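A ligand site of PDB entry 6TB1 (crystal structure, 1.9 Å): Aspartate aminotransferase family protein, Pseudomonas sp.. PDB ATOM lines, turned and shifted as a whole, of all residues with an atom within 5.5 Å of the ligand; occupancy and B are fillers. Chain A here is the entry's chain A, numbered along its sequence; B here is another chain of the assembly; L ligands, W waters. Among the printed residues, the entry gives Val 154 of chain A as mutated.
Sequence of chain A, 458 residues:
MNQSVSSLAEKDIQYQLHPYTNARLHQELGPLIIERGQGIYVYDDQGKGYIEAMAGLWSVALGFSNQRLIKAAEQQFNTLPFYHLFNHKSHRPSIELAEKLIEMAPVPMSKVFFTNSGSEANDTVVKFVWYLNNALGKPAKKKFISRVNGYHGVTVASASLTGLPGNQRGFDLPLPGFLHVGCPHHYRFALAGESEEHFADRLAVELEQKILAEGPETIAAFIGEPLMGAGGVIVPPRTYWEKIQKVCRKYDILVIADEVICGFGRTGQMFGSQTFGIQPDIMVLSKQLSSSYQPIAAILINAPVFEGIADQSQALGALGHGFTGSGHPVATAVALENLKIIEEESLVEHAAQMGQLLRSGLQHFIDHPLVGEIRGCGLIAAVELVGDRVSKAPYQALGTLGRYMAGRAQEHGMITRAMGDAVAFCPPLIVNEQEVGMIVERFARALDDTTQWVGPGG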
ATOM      1  N   ASN A 116      -3.877 -10.003 -18.681  1.00  0.00           N
ATOM      2  CA  ASN A 116      -3.436  -8.821 -19.481  1.00  0.00           C
ATOM      3  C   ASN A 116      -2.545  -7.919 -18.642  1.00  0.00           C
ATOM      4  O   ASN A 116      -1.568  -7.388 -19.195  1.00  0.00           O
ATOM      5  CB  ASN A 116      -4.612  -8.025 -20.042  1.00  0.00           C
ATOM      6  CG  ASN A 116      -5.606  -8.895 -20.777  1.00  0.00           C
ATOM      7  OD1 ASN A 116      -5.307  -9.424 -21.837  1.00  0.00           O
ATOM      8  ND2 ASN A 116      -6.788  -9.068 -20.186  1.00  0.00           N
ATOM      9  N   SER A 117      -2.871  -7.712 -17.350  1.00  0.00           N
ATOM     10  CA  SER A 117      -2.232  -6.672 -16.506  1.00  0.00           C
ATOM     11  C   SER A 117      -1.698  -7.230 -15.174  1.00  0.00           C
ATOM     12  O   SER A 117      -2.222  -8.258 -14.686  1.00  0.00           O
ATOM     13  CB  SER A 117      -3.192  -5.529 -16.254  1.00  0.00           C
ATOM     14  OG  SER A 117      -4.223  -5.915 -15.367  1.00  0.00           O
ATOM     15  N   GLY A 118      -0.757  -6.508 -14.566  1.00  0.00           N
ATOM     16  CA  GLY A 118      -0.291  -6.735 -13.193  1.00  0.00           C
ATOM     17  C   GLY A 118      -1.441  -6.640 -12.199  1.00  0.00           C
ATOM     18  O   GLY A 118      -1.483  -7.479 -11.266  1.00  0.00           O
ATOM     19  N   SER A 119      -2.338  -5.658 -12.368  1.00  0.00           N
ATOM     20  CA  SER A 119      -3.521  -5.475 -11.476  1.00  0.00           C
ATOM     21  C   SER A 119      -4.404  -6.732 -11.544  1.00  0.00           C
ATOM     22  O   SER A 119      -4.831  -7.225 -10.489  1.00  0.00           O
ATOM     23  CB  SER A 119      -4.320  -4.213 -11.798  1.00  0.00           C
ATOM     24  OG  SER A 119      -3.517  -3.032 -11.689  1.00  0.00           O
ATOM     25  N   GLU A 120      -4.737  -7.190 -12.746  1.00  0.00           N
ATOM     26  CA  GLU A 120      -5.539  -8.428 -12.951  1.00  0.00           C
ATOM     27  C   GLU A 120      -4.821  -9.624 -12.309  1.00  0.00           C
ATOM     28  O   GLU A 120      -5.521 -10.490 -11.704  1.00  0.00           O
ATOM     29  CB  GLU A 120      -5.732  -8.782 -14.417  1.00  0.00           C
ATOM     30  CG  GLU A 120      -6.783  -7.961 -15.171  1.00  0.00           C
ATOM     31  CD  GLU A 120      -6.663  -8.200 -16.679  1.00  0.00           C
ATOM     32  OE1 GLU A 120      -5.620  -8.748 -17.078  1.00  0.00           O
ATOM     33  OE2 GLU A 120      -7.606  -7.862 -17.441  1.00  0.00           O
ATOM     34  N   ASN A 122      -2.561  -9.778  -9.713  1.00  0.00           N
ATOM     35  CA  ASN A 122      -2.649  -9.728  -8.223  1.00  0.00           C
ATOM     36  C   ASN A 122      -4.097 -10.019  -7.787  1.00  0.00           C
ATOM     37  O   ASN A 122      -4.287 -10.755  -6.768  1.00  0.00           O
ATOM     38  CB  ASN A 122      -2.046  -8.437  -7.661  1.00  0.00           C
ATOM     39  CG  ASN A 122      -0.529  -8.471  -7.656  1.00  0.00           C
ATOM     40  OD1 ASN A 122       0.072  -9.532  -7.491  1.00  0.00           O
ATOM     41  ND2 ASN A 122       0.092  -7.324  -7.840  1.00  0.00           N
ATOM     42  N   TYR A 151       3.076  -1.060  -3.972  1.00  0.00           N
ATOM     43  CA  TYR A 151       2.197  -0.867  -5.152  1.00  0.00           C
ATOM     44  C   TYR A 151       1.953  -2.218  -5.817  1.00  0.00           C
ATOM     45  O   TYR A 151       2.933  -2.914  -6.164  1.00  0.00           O
ATOM     46  CB  TYR A 151       2.783   0.151  -6.142  1.00  0.00           C
ATOM     47  CG  TYR A 151       1.846   0.505  -7.285  1.00  0.00           C
ATOM     48  CD1 TYR A 151       0.757   1.321  -7.069  1.00  0.00           C
ATOM     49  CD2 TYR A 151       2.048   0.020  -8.580  1.00  0.00           C
ATOM     50  CE1 TYR A 151      -0.105   1.682  -8.102  1.00  0.00           C
ATOM     51  CE2 TYR A 151       1.184   0.364  -9.614  1.00  0.00           C
ATOM     52  CZ  TYR A 151       0.105   1.207  -9.381  1.00  0.00           C
ATOM     53  OH  TYR A 151      -0.741   1.600 -10.390  1.00  0.00           O
ATOM     54  N   HIS A 152       0.680  -2.586  -5.932  1.00  0.00           N
ATOM     55  CA  HIS A 152       0.238  -3.923  -6.427  1.00  0.00           C
ATOM     56  C   HIS A 152      -0.900  -3.755  -7.442  1.00  0.00           C
ATOM     57  O   HIS A 152      -1.453  -4.782  -7.871  1.00  0.00           O
ATOM     58  CB  HIS A 152      -0.149  -4.826  -5.229  1.00  0.00           C
ATOM     59  CG  HIS A 152       0.982  -5.046  -4.281  1.00  0.00           C
ATOM     60  ND1 HIS A 152       2.091  -5.792  -4.620  1.00  0.00           N
ATOM     61  CD2 HIS A 152       1.214  -4.552  -3.031  1.00  0.00           C
ATOM     62  CE1 HIS A 152       2.959  -5.766  -3.623  1.00  0.00           C
ATOM     63  NE2 HIS A 152       2.445  -5.010  -2.635  1.00  0.00           N
ATOM     64  N   GLY A 153      -1.223  -2.525  -7.860  1.00  0.00           N
ATOM     65  CA  GLY A 153      -2.222  -2.304  -8.923  1.00  0.00           C
ATOM     66  C   GLY A 153      -3.467  -1.609  -8.409  1.00  0.00           C
ATOM     67  O   GLY A 153      -3.473  -1.142  -7.242  1.00  0.00           O
ATOM     68  N   VAL A 154      -4.503  -1.541  -9.250  1.00  0.00           N
ATOM     69  CA  VAL A 154      -5.597  -0.532  -9.113  1.00  0.00           C
ATOM     70  C   VAL A 154      -6.995  -1.164  -9.173  1.00  0.00           C
ATOM     71  O   VAL A 154      -8.001  -0.385  -9.112  1.00  0.00           O
ATOM     72  CB  VAL A 154      -5.425   0.592 -10.155  1.00  0.00           C
ATOM     73  CG1 VAL A 154      -4.102   1.318  -9.992  1.00  0.00           C
ATOM     74  CG2 VAL A 154      -5.579   0.086 -11.587  1.00  0.00           C
ATOM     75  N   GLU A 225       6.798  -6.552  -3.033  1.00  0.00           N
ATOM     76  CA  GLU A 225       7.850  -6.275  -4.048  1.00  0.00           C
ATOM     77  C   GLU A 225       9.195  -6.503  -3.389  1.00  0.00           C
ATOM     78  O   GLU A 225       9.410  -6.026  -2.276  1.00  0.00           O
ATOM     79  CB  GLU A 225       7.757  -4.829  -4.497  1.00  0.00           C
ATOM     80  CG  GLU A 225       6.440  -4.403  -5.126  1.00  0.00           C
ATOM     81  CD  GLU A 225       6.298  -2.886  -5.119  1.00  0.00           C
ATOM     82  OE1 GLU A 225       6.784  -2.238  -6.082  1.00  0.00           O
ATOM     83  OE2 GLU A 225       5.798  -2.357  -4.075  1.00  0.00           O
ATOM     84  N   ALA A 230       7.178   1.943  -7.442  1.00  0.00           N
ATOM     85  CA  ALA A 230       6.357   3.177  -7.589  1.00  0.00           C
ATOM     86  C   ALA A 230       6.262   3.932  -6.249  1.00  0.00           C
ATOM     87  O   ALA A 230       6.098   5.168  -6.263  1.00  0.00           O
ATOM     88  CB  ALA A 230       4.987   2.814  -8.098  1.00  0.00           C
ATOM     89  N   ASP A 258       5.909  -9.998  -5.687  1.00  0.00           N
ATOM     90  CA  ASP A 258       5.414  -9.114  -6.775  1.00  0.00           C
ATOM     91  C   ASP A 258       6.632  -8.593  -7.538  1.00  0.00           C
ATOM     92  O   ASP A 258       7.256  -7.624  -7.061  1.00  0.00           O
ATOM     93  CB  ASP A 258       4.495  -8.005  -6.261  1.00  0.00           C
ATOM     94  CG  ASP A 258       3.878  -7.213  -7.417  1.00  0.00           C
ATOM     95  OD1 ASP A 258       4.410  -7.326  -8.544  1.00  0.00           O
ATOM     96  OD2 ASP A 258       2.853  -6.520  -7.199  1.00  0.00           O
ATOM     97  N   VAL A 260       6.653  -7.443 -10.678  1.00  0.00           N
ATOM     98  CA  VAL A 260       6.177  -6.747 -11.920  1.00  0.00           C
ATOM     99  C   VAL A 260       7.234  -5.720 -12.371  1.00  0.00           C
ATOM    100  O   VAL A 260       7.447  -5.619 -13.582  1.00  0.00           O
ATOM    101  CB  VAL A 260       4.774  -6.135 -11.710  1.00  0.00           C
ATOM    102  CG1 VAL A 260       4.450  -5.074 -12.756  1.00  0.00           C
ATOM    103  CG2 VAL A 260       3.706  -7.211 -11.681  1.00  0.00           C
ATOM    104  N   ILE A 261       7.931  -5.025 -11.449  1.00  0.00           N
ATOM    105  CA  ILE A 261       9.074  -4.129 -11.828  1.00  0.00           C
ATOM    106  C   ILE A 261      10.423  -4.884 -11.759  1.00  0.00           C
ATOM    107  O   ILE A 261      11.239  -4.710 -12.692  1.00  0.00           O
ATOM    108  CB  ILE A 261       9.081  -2.823 -10.999  1.00  0.00           C
ATOM    109  CG1 ILE A 261       7.991  -1.871 -11.511  1.00  0.00           C
ATOM    110  CG2 ILE A 261      10.458  -2.153 -11.029  1.00  0.00           C
ATOM    111  CD1 ILE A 261       7.791  -0.650 -10.654  1.00  0.00           C
ATOM    112  N   SER A 286       5.122  -8.917 -15.138  1.00  0.00           N
ATOM    113  CA  SER A 286       4.519  -8.096 -16.227  1.00  0.00           C
ATOM    114  C   SER A 286       5.584  -7.134 -16.761  1.00  0.00           C
ATOM    115  O   SER A 286       6.783  -7.426 -16.595  1.00  0.00           O
ATOM    116  CB  SER A 286       3.260  -7.356 -15.761  1.00  0.00           C
ATOM    117  OG  SER A 286       2.496  -6.883 -16.867  1.00  0.00           O
ATOM    118  N   LYS A 287       5.163  -6.025 -17.375  1.00  0.00           N
ATOM    119  CA  LYS A 287       6.041  -4.885 -17.755  1.00  0.00           C
ATOM    120  C   LYS A 287       7.229  -5.380 -18.612  1.00  0.00           C
ATOM    121  O   LYS A 287       7.021  -5.559 -19.825  1.00  0.00           O
ATOM    122  CB  LYS A 287       6.416  -4.094 -16.485  1.00  0.00           C
ATOM    123  CG  LYS A 287       5.324  -3.136 -15.975  1.00  0.00           C
ATOM    124  CD  LYS A 287       5.734  -2.244 -14.775  1.00  0.00           C
ATOM    125  CE  LYS A 287       4.695  -1.192 -14.342  1.00  0.00           C
ATOM    126  NZ  LYS A 287       3.988  -1.508 -13.067  1.00  0.00           N
ATOM    127  N   ASN B 116      -7.470  -2.669 -20.472  1.00  0.00           N
ATOM    128  CA  ASN B 116      -7.098  -3.847 -21.297  1.00  0.00           C
ATOM    129  C   ASN B 116      -8.317  -4.755 -21.497  1.00  0.00           C
ATOM    130  O   ASN B 116      -8.483  -5.313 -22.614  1.00  0.00           O
ATOM    131  CB  ASN B 116      -5.922  -4.627 -20.706  1.00  0.00           C
ATOM    132  CG  ASN B 116      -4.733  -3.754 -20.375  1.00  0.00           C
ATOM    133  OD1 ASN B 116      -4.062  -3.247 -21.276  1.00  0.00           O
ATOM    134  ND2 ASN B 116      -4.491  -3.538 -19.087  1.00  0.00           N
ATOM    135  N   GLU B 120     -11.626  -5.478 -16.161  1.00  0.00           N
ATOM    136  CA  GLU B 120     -10.976  -4.253 -15.637  1.00  0.00           C
ATOM    137  C   GLU B 120     -11.933  -3.066 -15.822  1.00  0.00           C
ATOM    138  O   GLU B 120     -11.978  -2.184 -14.932  1.00  0.00           O
ATOM    139  CB  GLU B 120      -9.694  -3.887 -16.380  1.00  0.00           C
ATOM    140  CG  GLU B 120      -8.448  -4.705 -16.015  1.00  0.00           C
ATOM    141  CD  GLU B 120      -7.345  -4.446 -17.022  1.00  0.00           C
ATOM    142  OE1 GLU B 120      -7.667  -3.911 -18.119  1.00  0.00           O
ATOM    143  OE2 GLU B 120      -6.164  -4.790 -16.747  1.00  0.00           O
ATOM    144  N   GLY B 322      -5.216   3.958 -12.892  1.00  0.00           N
ATOM    145  CA  GLY B 322      -4.745   3.736 -14.271  1.00  0.00           C
ATOM    146  C   GLY B 322      -4.012   2.422 -14.416  1.00  0.00           C
ATOM    147  O   GLY B 322      -3.339   2.016 -13.444  1.00  0.00           O
ATOM    148  N   PHE B 323      -4.123   1.793 -15.586  1.00  0.00           N
ATOM    149  CA  PHE B 323      -3.359   0.580 -15.957  1.00  0.00           C
ATOM    150  C   PHE B 323      -2.213   0.963 -16.882  1.00  0.00           C
ATOM    151  O   PHE B 323      -2.363   1.884 -17.704  1.00  0.00           O
ATOM    152  CB  PHE B 323      -4.280  -0.450 -16.593  1.00  0.00           C
ATOM    153  CG  PHE B 323      -5.484  -0.820 -15.761  1.00  0.00           C
ATOM    154  CD1 PHE B 323      -5.402  -1.836 -14.814  1.00  0.00           C
ATOM    155  CD2 PHE B 323      -6.702  -0.187 -15.946  1.00  0.00           C
ATOM    156  CE1 PHE B 323      -6.519  -2.197 -14.063  1.00  0.00           C
ATOM    157  CE2 PHE B 323      -7.814  -0.527 -15.173  1.00  0.00           C
ATOM    158  CZ  PHE B 323      -7.715  -1.538 -14.238  1.00  0.00           C
ATOM    159  N   THR B 324      -1.061   0.300 -16.745  1.00  0.00           N
ATOM    160  CA  THR B 324       0.117   0.462 -17.641  1.00  0.00           C
ATOM    161  C   THR B 324      -0.355   0.487 -19.107  1.00  0.00           C
ATOM    162  O   THR B 324       0.045   1.426 -19.862  1.00  0.00           O
ATOM    163  CB  THR B 324       1.169  -0.619 -17.381  1.00  0.00           C
ATOM    164  OG1 THR B 324       1.628  -0.477 -16.039  1.00  0.00           O
ATOM    165  CG2 THR B 324       2.367  -0.481 -18.300  1.00  0.00           C
ATOM    166  N   GLY B 325      -1.218  -0.454 -19.464  1.00  0.00           N
ATOM    167  CA  GLY B 325      -1.734  -0.647 -20.833  1.00  0.00           C
ATOM    168  C   GLY B 325      -2.883   0.267 -21.208  1.00  0.00           C
ATOM    169  O   GLY B 325      -3.314   0.166 -22.369  1.00  0.00           O
HETATM  170  N1  LIG L   1       2.708  -4.434  -9.217  1.00  0.00           N
HETATM  171  C1  LIG L   1       3.792  -3.670  -9.387  1.00  0.00           C
HETATM  172  C2  LIG L   1       4.980  -3.869  -8.485  1.00  0.00           C
HETATM  173  C3  LIG L   1       3.837  -2.719 -10.419  1.00  0.00           C
HETATM  174  O1  LIG L   1       4.945  -1.944 -10.531  1.00  0.00           O
HETATM  175  C4  LIG L   1       2.745  -2.578 -11.300  1.00  0.00           C
HETATM  176  C5  LIG L   1       2.853  -1.600 -12.398  1.00  0.00           C
HETATM  177  C6  LIG L   1       1.602  -3.380 -11.085  1.00  0.00           C
HETATM  178  C7  LIG L   1       1.636  -4.271 -10.031  1.00  0.00           C
HETATM  179  C8  LIG L   1       0.336  -3.225 -11.901  1.00  0.00           C
HETATM  180  O2  LIG L   1       0.457  -3.404 -13.341  1.00  0.00           O
HETATM  181  P1  LIG L   1      -0.684  -2.861 -14.395  1.00  0.00           P
HETATM  182  O3  LIG L   1      -0.408  -1.366 -14.534  1.00  0.00           O
HETATM  183  O4  LIG L   1      -2.050  -3.197 -13.859  1.00  0.00           O
HETATM  184  O5  LIG L   1      -0.323  -3.649 -15.669  1.00  0.00           O
HETATM  185  O   HOH W   1       1.664  -4.381 -17.452  1.00  0.00           O
HETATM  186  O   HOH W   2       5.752  -0.537  -8.136  1.00  0.00           O
HETATM  187  O   HOH W   3      -0.813   0.696 -12.946  1.00  0.00           O
HETATM  188  O   HOH W   4      -1.719  -2.900 -17.953  1.00  0.00           O
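A carbon (C5) of the ligand is bonded to the side-chain amino group (NZ) of Lys 287. An oxygen (O4) of the ligand sits at hydrogen-bond distance from the backbone NH of Ser 119, at 2.9 Å. The side-chain hydroxyl (OG) of Ser 119 sits at hydrogen-bond distance from an oxygen (O4) of the ligand, at 2.6 Å. An oxygen (O3) of the ligand is in hydrogen-bond range of the backbone NH of Thr 324 of chain B. OG1 of Thr 324 of chain B lies within hydrogen-bond range of O3 of the ligand (2.7 Å). The backbone NH (N) of Gly 118 is in hydrogen-bond range of an oxygen (O5) of the ligand.
OG of Ser 119 lies within hydrogen-bond range of N of Val 154. OD1 of Asp 258 is in hydrogen-bond range of N of Val 260. The side-chain carboxylate of Asp 258 sits at hydrogen-bond distance from a ring nitrogen (ND1) of His 152 (2.8 Å). The side-chain carboxylate (OD2) of Asp 258 lies within hydrogen-bond range of the side-chain amide nitrogen (ND2) of Asn 122, 2.9 Å away. The backbone NH of Tyr 151 is in hydrogen-bond range of the side-chain carboxylate of Glu 225. OE1 of Glu 120 of chain A sits at hydrogen-bond distance from N of Ser 117, at 3.0 Å. The side-chain carboxylate (OE2) of Glu 120 of chain B lies within hydrogen-bond range of the side-chain hydroxyl (OG) of Ser 117 (2.6 Å). The backbone carbonyl oxygen (O) of His 152 is in hydrogen-bond range of the side-chain amide nitrogen (ND2) of Asn 122 (3.0 Å).
O of Tyr 151 sits close to N1 of the ligand. The side-chain carboxylate of Asp 258 lies close to a nitrogen (N1) of the ligand. Ser 117 touches the ligand (CB to O5, 3.5 Å). His 152 touches the ligand (C to C7, 3.7 Å). Gly 153 touches the ligand (N to C7, 3.99 Å). Glu 225 touches the ligand (OE1 to C2, 3.4 Å). Val 260 touches the ligand (CG1 to C4, 3.4 Å). CD1 of Ile 261 touches O1 of the ligand, 3.1 Å away. CD1 of Phe 323 of chain B touches O4 of the ligand, at 3.7 Å. Hydrophobic or aromatic side chains that line the ligand: Tyr 151, Val 260, Ile 261 and Phe 323 of chain B. Of the 23 residues printed, 13 come within 4 Å of the ligand. The nearest printed residue that does not touch the ligand is Asn 122 (4.1 Å).
Water W3 lies within hydrogen-bond range of O3 of the ligand (2.6 Å), OH of Tyr 151 (2.7 Å) and O of Gly 322 of chain B (2.9 Å). Water W1 lies within hydrogen-bond range of the side-chain hydroxyl (OG) of Ser 286 (2.7 Å) and an oxygen (O5) of the ligand (2.8 Å). Water W2 lies within hydrogen-bond range of the side-chain carboxylate (OE1) of Glu 225 (2.9 Å), an oxygen (O1) of the ligand (2.9 Å) and the backbone NH (N) of Ala 230 (2.9 Å).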
